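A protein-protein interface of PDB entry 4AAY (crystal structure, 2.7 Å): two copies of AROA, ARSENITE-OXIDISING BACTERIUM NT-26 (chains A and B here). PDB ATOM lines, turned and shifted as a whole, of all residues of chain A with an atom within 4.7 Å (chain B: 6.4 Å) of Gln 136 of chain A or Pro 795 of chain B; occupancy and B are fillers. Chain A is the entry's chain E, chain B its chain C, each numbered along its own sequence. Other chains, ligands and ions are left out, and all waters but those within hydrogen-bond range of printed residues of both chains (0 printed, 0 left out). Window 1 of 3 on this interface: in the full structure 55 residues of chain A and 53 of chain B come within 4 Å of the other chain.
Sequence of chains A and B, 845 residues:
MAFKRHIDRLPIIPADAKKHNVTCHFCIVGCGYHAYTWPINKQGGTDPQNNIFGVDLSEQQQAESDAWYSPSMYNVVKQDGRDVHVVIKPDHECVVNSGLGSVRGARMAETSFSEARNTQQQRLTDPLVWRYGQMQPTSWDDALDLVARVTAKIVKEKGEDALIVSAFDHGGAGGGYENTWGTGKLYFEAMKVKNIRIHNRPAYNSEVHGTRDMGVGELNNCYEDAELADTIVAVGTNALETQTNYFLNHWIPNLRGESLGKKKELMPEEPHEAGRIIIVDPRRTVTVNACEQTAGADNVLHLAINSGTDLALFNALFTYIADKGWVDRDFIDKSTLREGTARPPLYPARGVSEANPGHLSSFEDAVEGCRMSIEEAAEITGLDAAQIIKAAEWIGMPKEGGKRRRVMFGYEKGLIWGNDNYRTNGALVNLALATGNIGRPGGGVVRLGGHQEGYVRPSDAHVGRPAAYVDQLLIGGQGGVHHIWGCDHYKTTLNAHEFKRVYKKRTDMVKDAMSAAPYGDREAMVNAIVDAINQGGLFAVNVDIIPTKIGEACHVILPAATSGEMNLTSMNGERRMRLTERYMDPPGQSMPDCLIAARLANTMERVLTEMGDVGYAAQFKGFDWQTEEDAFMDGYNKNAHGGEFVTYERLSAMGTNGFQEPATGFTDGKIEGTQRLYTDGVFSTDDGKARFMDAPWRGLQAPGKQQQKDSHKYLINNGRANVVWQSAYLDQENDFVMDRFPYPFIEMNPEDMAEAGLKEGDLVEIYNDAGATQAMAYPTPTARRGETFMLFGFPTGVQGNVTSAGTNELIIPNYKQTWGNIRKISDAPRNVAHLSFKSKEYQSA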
ATOM      1  N   PRO A 127      20.225  35.709  24.104  1.00  0.00           N
ATOM      2  CA  PRO A 127      19.921  36.569  22.976  1.00  0.00           C
ATOM      3  C   PRO A 127      19.076  35.835  21.944  1.00  0.00           C
ATOM      4  O   PRO A 127      19.295  34.642  21.691  1.00  0.00           O
ATOM      5  CB  PRO A 127      21.298  36.890  22.400  1.00  0.00           C
ATOM      6  CG  PRO A 127      22.233  36.714  23.564  1.00  0.00           C
ATOM      7  CD  PRO A 127      21.676  35.539  24.290  1.00  0.00           C
ATOM      8  N   LEU A 128      18.106  36.546  21.373  1.00  0.00           N
ATOM      9  CA  LEU A 128      17.249  35.986  20.340  1.00  0.00           C
ATOM     10  C   LEU A 128      17.393  36.817  19.058  1.00  0.00           C
ATOM     11  O   LEU A 128      17.598  38.030  19.100  1.00  0.00           O
ATOM     12  CB  LEU A 128      15.800  35.945  20.806  1.00  0.00           C
ATOM     13  CG  LEU A 128      15.382  35.267  22.139  1.00  0.00           C
ATOM     14  CD1 LEU A 128      13.942  35.620  22.512  1.00  0.00           C
ATOM     15  CD2 LEU A 128      15.544  33.747  22.089  1.00  0.00           C
ATOM     16  N   VAL A 129      17.342  36.154  17.912  1.00  0.00           N
ATOM     17  CA  VAL A 129      17.402  36.826  16.636  1.00  0.00           C
ATOM     18  C   VAL A 129      16.310  36.266  15.737  1.00  0.00           C
ATOM     19  O   VAL A 129      16.056  35.053  15.733  1.00  0.00           O
ATOM     20  CB  VAL A 129      18.765  36.629  15.964  1.00  0.00           C
ATOM     21  CG1 VAL A 129      18.746  37.183  14.542  1.00  0.00           C
ATOM     22  CG2 VAL A 129      19.850  37.286  16.813  1.00  0.00           C
ATOM     23  N   ARG A 131      15.231  34.724  12.669  1.00  0.00           N
ATOM     24  CA  ARG A 131      15.728  34.014  11.479  1.00  0.00           C
ATOM     25  C   ARG A 131      15.077  32.665  11.280  1.00  0.00           C
ATOM     26  O   ARG A 131      14.558  32.087  12.199  1.00  0.00           O
ATOM     27  CB  ARG A 131      17.229  33.821  11.549  1.00  0.00           C
ATOM     28  CG  ARG A 131      17.736  33.147  12.820  1.00  0.00           C
ATOM     29  CD  ARG A 131      19.238  32.948  12.687  1.00  0.00           C
ATOM     30  NE  ARG A 131      19.843  32.173  13.763  1.00  0.00           N
ATOM     31  CZ  ARG A 131      20.765  32.621  14.620  1.00  0.00           C
ATOM     32  NH1 ARG A 131      21.207  33.878  14.568  1.00  0.00           N
ATOM     33  NH2 ARG A 131      21.252  31.803  15.552  1.00  0.00           N
ATOM     34  N   TYR A 132      15.113  32.185  10.050  1.00  0.00           N
ATOM     35  CA  TYR A 132      14.530  30.911   9.688  1.00  0.00           C
ATOM     36  C   TYR A 132      13.013  30.866   9.943  1.00  0.00           C
ATOM     37  O   TYR A 132      12.445  29.788  10.170  1.00  0.00           O
ATOM     38  CB  TYR A 132      15.223  29.779  10.456  1.00  0.00           C
ATOM     39  CG  TYR A 132      16.726  29.829  10.411  1.00  0.00           C
ATOM     40  CD1 TYR A 132      17.390  30.048   9.215  1.00  0.00           C
ATOM     41  CD2 TYR A 132      17.484  29.659  11.566  1.00  0.00           C
ATOM     42  CE1 TYR A 132      18.769  30.110   9.161  1.00  0.00           C
ATOM     43  CE2 TYR A 132      18.859  29.712  11.523  1.00  0.00           C
ATOM     44  CZ  TYR A 132      19.496  29.939  10.317  1.00  0.00           C
ATOM     45  OH  TYR A 132      20.868  29.985  10.247  1.00  0.00           O
ATOM     46  N   GLN A 134      11.232  32.515  12.418  1.00  0.00           N
ATOM     47  CA  GLN A 134      10.788  32.804  13.780  1.00  0.00           C
ATOM     48  C   GLN A 134      11.942  33.351  14.602  1.00  0.00           C
ATOM     49  O   GLN A 134      13.052  33.497  14.104  1.00  0.00           O
ATOM     50  CB  GLN A 134      10.217  31.541  14.439  1.00  0.00           C
ATOM     51  CG  GLN A 134      11.256  30.465  14.539  1.00  0.00           C
ATOM     52  CD  GLN A 134      10.800  29.179  13.945  1.00  0.00           C
ATOM     53  OE1 GLN A 134      11.393  28.703  12.938  1.00  0.00           O
ATOM     54  NE2 GLN A 134       9.735  28.586  14.542  1.00  0.00           N
ATOM     55  N   MET A 135      11.663  33.682  15.858  1.00  0.00           N
ATOM     56  CA  MET A 135      12.705  34.098  16.795  1.00  0.00           C
ATOM     57  C   MET A 135      13.463  32.870  17.203  1.00  0.00           C
ATOM     58  O   MET A 135      12.870  31.841  17.446  1.00  0.00           O
ATOM     59  CB  MET A 135      12.107  34.792  18.021  1.00  0.00           C
ATOM     60  CG  MET A 135      11.589  36.196  17.732  1.00  0.00           C
ATOM     61  SD  MET A 135      12.937  37.370  17.360  1.00  0.00           S
ATOM     62  CE  MET A 135      12.437  37.568  15.698  1.00  0.00           C
ATOM     63  N   GLN A 136      14.788  32.982  17.224  1.00  0.00           N
ATOM     64  CA  GLN A 136      15.679  31.861  17.544  1.00  0.00           C
ATOM     65  C   GLN A 136      16.775  32.275  18.531  1.00  0.00           C
ATOM     66  O   GLN A 136      17.349  33.357  18.406  1.00  0.00           O
ATOM     67  CB  GLN A 136      16.355  31.342  16.282  1.00  0.00           C
ATOM     68  CG  GLN A 136      15.419  30.759  15.226  1.00  0.00           C
ATOM     69  CD  GLN A 136      14.946  29.350  15.520  1.00  0.00           C
ATOM     70  OE1 GLN A 136      15.521  28.377  15.003  1.00  0.00           O
ATOM     71  NE2 GLN A 136      13.883  29.224  16.315  1.00  0.00           N
ATOM     72  N   PRO A 137      17.101  31.402  19.494  1.00  0.00           N
ATOM     73  CA  PRO A 137      18.170  31.761  20.404  1.00  0.00           C
ATOM     74  C   PRO A 137      19.531  31.668  19.731  1.00  0.00           C
ATOM     75  O   PRO A 137      19.704  30.930  18.769  1.00  0.00           O
ATOM     76  CB  PRO A 137      18.048  30.739  21.536  1.00  0.00           C
ATOM     77  CG  PRO A 137      17.338  29.586  20.946  1.00  0.00           C
ATOM     78  CD  PRO A 137      16.603  30.043  19.722  1.00  0.00           C
ATOM     79  N   THR A 138      20.487  32.432  20.252  1.00  0.00           N
ATOM     80  CA  THR A 138      21.840  32.414  19.732  1.00  0.00           C
ATOM     81  C   THR A 138      22.796  32.888  20.796  1.00  0.00           C
ATOM     82  O   THR A 138      22.394  33.146  21.934  1.00  0.00           O
ATOM     83  CB  THR A 138      21.939  33.285  18.461  1.00  0.00           C
ATOM     84  OG1 THR A 138      23.179  33.026  17.784  1.00  0.00           O
ATOM     85  CG2 THR A 138      21.812  34.768  18.779  1.00  0.00           C
ATOM     86  N   LYS B 491       6.579  24.222  13.353  1.00  0.00           N
ATOM     87  CA  LYS B 491       7.649  23.343  13.800  1.00  0.00           C
ATOM     88  C   LYS B 491       7.708  22.005  13.055  1.00  0.00           C
ATOM     89  O   LYS B 491       8.758  21.402  12.987  1.00  0.00           O
ATOM     90  CB  LYS B 491       7.520  23.076  15.305  1.00  0.00           C
ATOM     91  CG  LYS B 491       7.774  24.311  16.166  1.00  0.00           C
ATOM     92  CD  LYS B 491       7.711  24.001  17.652  1.00  0.00           C
ATOM     93  CE  LYS B 491       6.287  23.805  18.134  1.00  0.00           C
ATOM     94  NZ  LYS B 491       6.213  23.193  19.495  1.00  0.00           N
ATOM     95  N   LYS B 549       3.650  28.092  17.959  1.00  0.00           N
ATOM     96  CA  LYS B 549       4.394  28.883  16.993  1.00  0.00           C
ATOM     97  C   LYS B 549       3.502  29.408  15.881  1.00  0.00           C
ATOM     98  O   LYS B 549       3.488  30.603  15.607  1.00  0.00           O
ATOM     99  CB  LYS B 549       5.569  28.092  16.401  1.00  0.00           C
ATOM    100  CG  LYS B 549       6.692  27.804  17.392  1.00  0.00           C
ATOM    101  CD  LYS B 549       7.149  29.045  18.172  1.00  0.00           C
ATOM    102  CE  LYS B 549       8.407  28.754  18.991  1.00  0.00           C
ATOM    103  NZ  LYS B 549       8.668  29.756  20.052  1.00  0.00           N
ATOM    104  N   GLN B 726       7.644  14.990  21.044  1.00  0.00           N
ATOM    105  CA  GLN B 726       7.105  15.709  19.870  1.00  0.00           C
ATOM    106  C   GLN B 726       7.798  17.073  19.669  1.00  0.00           C
ATOM    107  O   GLN B 726       9.019  17.151  19.754  1.00  0.00           O
ATOM    108  CB  GLN B 726       5.578  15.832  20.002  1.00  0.00           C
ATOM    109  CG  GLN B 726       4.870  14.501  19.861  1.00  0.00           C
ATOM    110  CD  GLN B 726       4.892  14.034  18.427  1.00  0.00           C
ATOM    111  OE1 GLN B 726       5.770  13.256  18.016  1.00  0.00           O
ATOM    112  NE2 GLN B 726       3.987  14.572  17.634  1.00  0.00           N
ATOM    113  N   SER B 727       7.026  18.130  19.420  1.00  0.00           N
ATOM    114  CA  SER B 727       7.586  19.456  19.163  1.00  0.00           C
ATOM    115  C   SER B 727       7.869  20.254  20.449  1.00  0.00           C
ATOM    116  O   SER B 727       7.930  21.487  20.417  1.00  0.00           O
ATOM    117  CB  SER B 727       6.646  20.269  18.262  1.00  0.00           C
ATOM    118  OG  SER B 727       5.465  20.645  18.950  1.00  0.00           O
ATOM    119  N   ALA B 728       8.036  19.547  21.564  1.00  0.00           N
ATOM    120  CA  ALA B 728       8.424  20.167  22.851  1.00  0.00           C
ATOM    121  C   ALA B 728       7.412  21.190  23.328  1.00  0.00           C
ATOM    122  O   ALA B 728       7.760  22.147  24.012  1.00  0.00           O
ATOM    123  CB  ALA B 728       9.811  20.784  22.776  1.00  0.00           C
ATOM    124  N   TYR B 729       6.149  20.982  22.964  1.00  0.00           N
ATOM    125  CA  TYR B 729       5.093  21.922  23.340  1.00  0.00           C
ATOM    126  C   TYR B 729       4.928  22.021  24.856  1.00  0.00           C
ATOM    127  O   TYR B 729       4.789  23.113  25.381  1.00  0.00           O
ATOM    128  CB  TYR B 729       3.770  21.607  22.648  1.00  0.00           C
ATOM    129  CG  TYR B 729       3.132  20.282  22.933  1.00  0.00           C
ATOM    130  CD1 TYR B 729       2.251  20.125  24.005  1.00  0.00           C
ATOM    131  CD2 TYR B 729       3.349  19.196  22.098  1.00  0.00           C
ATOM    132  CE1 TYR B 729       1.639  18.910  24.248  1.00  0.00           C
ATOM    133  CE2 TYR B 729       2.751  17.980  22.336  1.00  0.00           C
ATOM    134  CZ  TYR B 729       1.891  17.847  23.403  1.00  0.00           C
ATOM    135  OH  TYR B 729       1.278  16.638  23.653  1.00  0.00           O
ATOM    136  N   GLN B 732       9.133  22.615  26.487  1.00  0.00           N
ATOM    137  CA  GLN B 732       9.766  23.937  26.477  1.00  0.00           C
ATOM    138  C   GLN B 732       9.575  24.674  27.807  1.00  0.00           C
ATOM    139  O   GLN B 732      10.356  25.565  28.124  1.00  0.00           O
ATOM    140  CB  GLN B 732       9.288  24.794  25.310  1.00  0.00           C
ATOM    141  CG  GLN B 732       7.809  25.166  25.323  1.00  0.00           C
ATOM    142  CD  GLN B 732       7.352  25.815  24.030  1.00  0.00           C
ATOM    143  OE1 GLN B 732       8.133  26.012  23.108  1.00  0.00           O
ATOM    144  NE2 GLN B 732       6.080  26.144  23.959  1.00  0.00           N
ATOM    145  N   MET B 738      14.727  20.958  28.895  1.00  0.00           N
ATOM    146  CA  MET B 738      15.453  22.101  28.275  1.00  0.00           C
ATOM    147  C   MET B 738      16.890  22.282  28.792  1.00  0.00           C
ATOM    148  O   MET B 738      17.744  22.844  28.097  1.00  0.00           O
ATOM    149  CB  MET B 738      14.689  23.416  28.432  1.00  0.00           C
ATOM    150  CG  MET B 738      13.363  23.476  27.674  1.00  0.00           C
ATOM    151  SD  MET B 738      13.446  23.151  25.887  1.00  0.00           S
ATOM    152  CE  MET B 738      12.646  21.553  25.789  1.00  0.00           C
ATOM    153  N   TYR B 743      19.214  23.701  22.516  1.00  0.00           N
ATOM    154  CA  TYR B 743      19.096  23.650  21.059  1.00  0.00           C
ATOM    155  C   TYR B 743      18.846  22.208  20.634  1.00  0.00           C
ATOM    156  O   TYR B 743      19.208  21.284  21.361  1.00  0.00           O
ATOM    157  CB  TYR B 743      20.378  24.128  20.404  1.00  0.00           C
ATOM    158  CG  TYR B 743      20.779  25.541  20.762  1.00  0.00           C
ATOM    159  CD1 TYR B 743      21.530  25.797  21.884  1.00  0.00           C
ATOM    160  CD2 TYR B 743      20.403  26.620  19.960  1.00  0.00           C
ATOM    161  CE1 TYR B 743      21.894  27.095  22.201  1.00  0.00           C
ATOM    162  CE2 TYR B 743      20.762  27.919  20.273  1.00  0.00           C
ATOM    163  CZ  TYR B 743      21.510  28.149  21.379  1.00  0.00           C
ATOM    164  OH  TYR B 743      21.881  29.432  21.698  1.00  0.00           O
ATOM    165  N   PRO B 744      18.239  21.995  19.453  1.00  0.00           N
ATOM    166  CA  PRO B 744      18.194  20.639  18.960  1.00  0.00           C
ATOM    167  C   PRO B 744      19.578  20.193  18.570  1.00  0.00           C
ATOM    168  O   PRO B 744      20.344  20.980  18.031  1.00  0.00           O
ATOM    169  CB  PRO B 744      17.324  20.744  17.720  1.00  0.00           C
ATOM    170  CG  PRO B 744      17.546  22.112  17.223  1.00  0.00           C
ATOM    171  CD  PRO B 744      17.789  22.962  18.439  1.00  0.00           C
ATOM    172  N   THR B 773      18.117  26.342   8.678  1.00  0.00           N
ATOM    173  CA  THR B 773      17.779  26.199  10.075  1.00  0.00           C
ATOM    174  C   THR B 773      19.042  26.033  10.911  1.00  0.00           C
ATOM    175  O   THR B 773      20.159  26.046  10.378  1.00  0.00           O
ATOM    176  CB  THR B 773      16.844  24.998  10.277  1.00  0.00           C
ATOM    177  OG1 THR B 773      16.275  25.055  11.586  1.00  0.00           O
ATOM    178  CG2 THR B 773      17.588  23.693  10.073  1.00  0.00           C
ATOM    179  N   GLN B 774      18.867  25.894  12.214  1.00  0.00           N
ATOM    180  CA  GLN B 774      20.008  25.832  13.117  1.00  0.00           C
ATOM    181  C   GLN B 774      19.935  24.613  14.012  1.00  0.00           C
ATOM    182  O   GLN B 774      18.863  24.096  14.271  1.00  0.00           O
ATOM    183  CB  GLN B 774      20.111  27.103  13.961  1.00  0.00           C
ATOM    184  CG  GLN B 774      18.930  27.386  14.865  1.00  0.00           C
ATOM    185  CD  GLN B 774      19.142  28.645  15.704  1.00  0.00           C
ATOM    186  OE1 GLN B 774      19.731  29.626  15.231  1.00  0.00           O
ATOM    187  NE2 GLN B 774      18.664  28.617  16.961  1.00  0.00           N
ATOM    188  N   PHE B 792      13.971  16.466  15.243  1.00  0.00           N
ATOM    189  CA  PHE B 792      12.929  17.146  14.475  1.00  0.00           C
ATOM    190  C   PHE B 792      12.014  17.952  15.393  1.00  0.00           C
ATOM    191  O   PHE B 792      12.061  17.821  16.595  1.00  0.00           O
ATOM    192  CB  PHE B 792      12.073  16.133  13.705  1.00  0.00           C
ATOM    193  CG  PHE B 792      10.755  15.843  14.358  1.00  0.00           C
ATOM    194  CD1 PHE B 792      10.699  15.140  15.553  1.00  0.00           C
ATOM    195  CD2 PHE B 792       9.574  16.324  13.804  1.00  0.00           C
ATOM    196  CE1 PHE B 792       9.484  14.892  16.173  1.00  0.00           C
ATOM    197  CE2 PHE B 792       8.356  16.085  14.422  1.00  0.00           C
ATOM    198  CZ  PHE B 792       8.310  15.361  15.598  1.00  0.00           C
ATOM    199  N   GLY B 793      11.168  18.771  14.806  1.00  0.00           N
ATOM    200  CA  GLY B 793      10.083  19.446  15.526  1.00  0.00           C
ATOM    201  C   GLY B 793      10.421  20.468  16.602  1.00  0.00           C
ATOM    202  O   GLY B 793       9.522  20.941  17.289  1.00  0.00           O
ATOM    203  N   PHE B 794      11.683  20.849  16.729  1.00  0.00           N
ATOM    204  CA  PHE B 794      12.141  21.525  17.937  1.00  0.00           C
ATOM    205  C   PHE B 794      12.070  23.043  17.821  1.00  0.00           C
ATOM    206  O   PHE B 794      12.572  23.623  16.850  1.00  0.00           O
ATOM    207  CB  PHE B 794      13.570  21.091  18.267  1.00  0.00           C
ATOM    208  CG  PHE B 794      13.853  21.007  19.742  1.00  0.00           C
ATOM    209  CD1 PHE B 794      13.247  20.032  20.528  1.00  0.00           C
ATOM    210  CD2 PHE B 794      14.713  21.892  20.339  1.00  0.00           C
ATOM    211  CE1 PHE B 794      13.500  19.946  21.877  1.00  0.00           C
ATOM    212  CE2 PHE B 794      14.976  21.811  21.693  1.00  0.00           C
ATOM    213  CZ  PHE B 794      14.361  20.843  22.467  1.00  0.00           C
ATOM    214  N   PRO B 795      11.474  23.706  18.833  1.00  0.00           N
ATOM    215  CA  PRO B 795      11.225  25.148  18.717  1.00  0.00           C
ATOM    216  C   PRO B 795      12.481  25.989  18.514  1.00  0.00           C
ATOM    217  O   PRO B 795      12.392  27.048  17.917  1.00  0.00           O
ATOM    218  CB  PRO B 795      10.542  25.507  20.045  1.00  0.00           C
ATOM    219  CG  PRO B 795      10.887  24.411  20.974  1.00  0.00           C
ATOM    220  CD  PRO B 795      10.962  23.178  20.108  1.00  0.00           C
ATOM    221  N   THR B 796      13.636  25.532  18.977  1.00  0.00           N
ATOM    222  CA  THR B 796      14.843  26.366  18.900  1.00  0.00           C
ATOM    223  C   THR B 796      15.710  26.005  17.680  1.00  0.00           C
ATOM    224  O   THR B 796      16.860  26.443  17.557  1.00  0.00           O
ATOM    225  CB  THR B 796      15.647  26.281  20.215  1.00  0.00           C
ATOM    226  OG1 THR B 796      15.885  24.902  20.514  1.00  0.00           O
ATOM    227  CG2 THR B 796      14.849  26.927  21.397  1.00  0.00           C
ATOM    228  N   GLY B 797      15.135  25.241  16.759  1.00  0.00           N
ATOM    229  CA  GLY B 797      15.811  24.851  15.517  1.00  0.00           C
ATOM    230  C   GLY B 797      14.975  23.807  14.815  1.00  0.00           C
ATOM    231  O   GLY B 797      14.960  22.657  15.221  1.00  0.00           O
ATOM    232  N   VAL B 798      14.234  24.221  13.799  1.00  0.00           N
ATOM    233  CA  VAL B 798      13.225  23.383  13.170  1.00  0.00           C
ATOM    234  C   VAL B 798      13.813  22.726  11.932  1.00  0.00           C
ATOM    235  O   VAL B 798      14.135  23.418  10.977  1.00  0.00           O
ATOM    236  CB  VAL B 798      12.004  24.228  12.754  1.00  0.00           C
ATOM    237  CG1 VAL B 798      10.990  23.398  11.964  1.00  0.00           C
ATOM    238  CG2 VAL B 798      11.344  24.845  13.987  1.00  0.00           C
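O of Pro 137 of chain A lies within hydrogen-bond range of NE2 of Gln 774 of chain B (3.1 Å).
NE2 of Gln 136 of chain A is in hydrogen-bond range of O of Pro 795 of chain B.
O of Thr 796 of chain B sits close to OE1 of Gln 136 of chain A (3.5 Å).
The side-chain amide oxygen (OE1) of Gln 774 of chain B is in hydrogen-bond range of the guanidinium group (NH2) of Arg 131 of chain A, at 2.7 Å.
The side-chain hydroxyl (OG1) of Thr 138 of chain A is in hydrogen-bond range of the guanidinium group (NH2) of Arg 131 of chain A (3.2 Å).
The side-chain amide nitrogen (NE2) of Gln 774 of chain B is in hydrogen-bond range of the backbone carbonyl oxygen (O) of Thr 796 of chain B (2.9 Å).
The side-chain hydroxyl (OG1) of Thr 773 of chain B is in hydrogen-bond range of the backbone carbonyl oxygen (O) of Val 798 of chain B (2.8 Å).
The backbone carbonyl oxygen (O) of Pro 127 of chain A sits at hydrogen-bond distance from the backbone NH (N) of Thr 138 of chain A, 2.9 Å away.
OE1 of Gln 134 of chain A lies close to O of Tyr 132 of chain A, at 3.2 Å.
The backbone NH (N) of Val 129 of chain A lies within hydrogen-bond range of the backbone carbonyl oxygen (O) of Gln 136 of chain A (2.8 Å).
Among the printed residues, pairs that only touch across the chains: Pro 137 of chain A with Tyr 743 of chain B (3.5 Å), Gln 136 of chain A with Gln 774 of chain B (3.6 Å), Thr 138 of chain A with Tyr 743 of chain B (3.6 Å), Gln 136 of chain A with Gly 797 of chain B (3.6 Å), Pro 137 of chain A with Thr 796 of chain B (3.7 Å), Tyr 132 of chain A with Thr 773 of chain B (3.7 Å), Tyr 132 of chain A with Gln 774 of chain B (3.8 Å) and Gln 134 of chain A with Val 798 of chain B (3.998 Å).
Printed residues of chain B within 4 Å of Gln 134 of chain A: Val 798 (3.998 Å).
Gln 136 of chain A touches just these residues of chain B: Gln 774 (3.6 Å), Pro 795 (3.1 Å), Thr 796 (3.5 Å) and Gly 797 (3.6 Å).
Printed residues of chain B within 4 Å of Pro 137 of chain A: Tyr 743, Gln 774 and Thr 796.
Printed residues of chain A within 4 Å of Tyr 743 of chain B: Pro 137 and Thr 138.
Of the printed residues of chain A, Gly 797 of chain B touches Gln 136.
Of the printed residues of chain A, Val 798 of chain B touches Gln 134.
The nearest residue of chain B that does not touch Gln 136 of chain A is Val 798 of chain B (4.5 Å).
The nearest residue of chain A that does not touch Pro 795 of chain B is Gln 134 of chain A (4.6 Å).
The nearest printed residue of chain B that does not touch Tyr 132 of chain A is Val 798 of chain B (6.1 Å).
Of the 19 printed residues of chain B, 7 touch a printed residue of chain A.
Hydrophobic or aromatic side chains of chain B that line the printed part of chain A: Tyr 743 and Val 798.
Along chain B the printed residues that touch a printed residue of chain A span positions 743 to 798.
Printed residues of chain A that touch a printed residue of chain B: Arg 131, Tyr 132, Gln 134, Gln 136, Pro 137 and Thr 138.
Hydrophobic or aromatic side chains of chain A that line the printed part of chain B: Tyr 132 and Pro 137.
Among the printed residues, no Asp or Glu carboxylate lies within 4 Å of a Lys or Arg side-chain nitrogen of the other chain.
No position is printed for both chains.
Of the 12 pairs that touch across the chains among the printed residues, none has its exchanged pair printed and touching as well.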
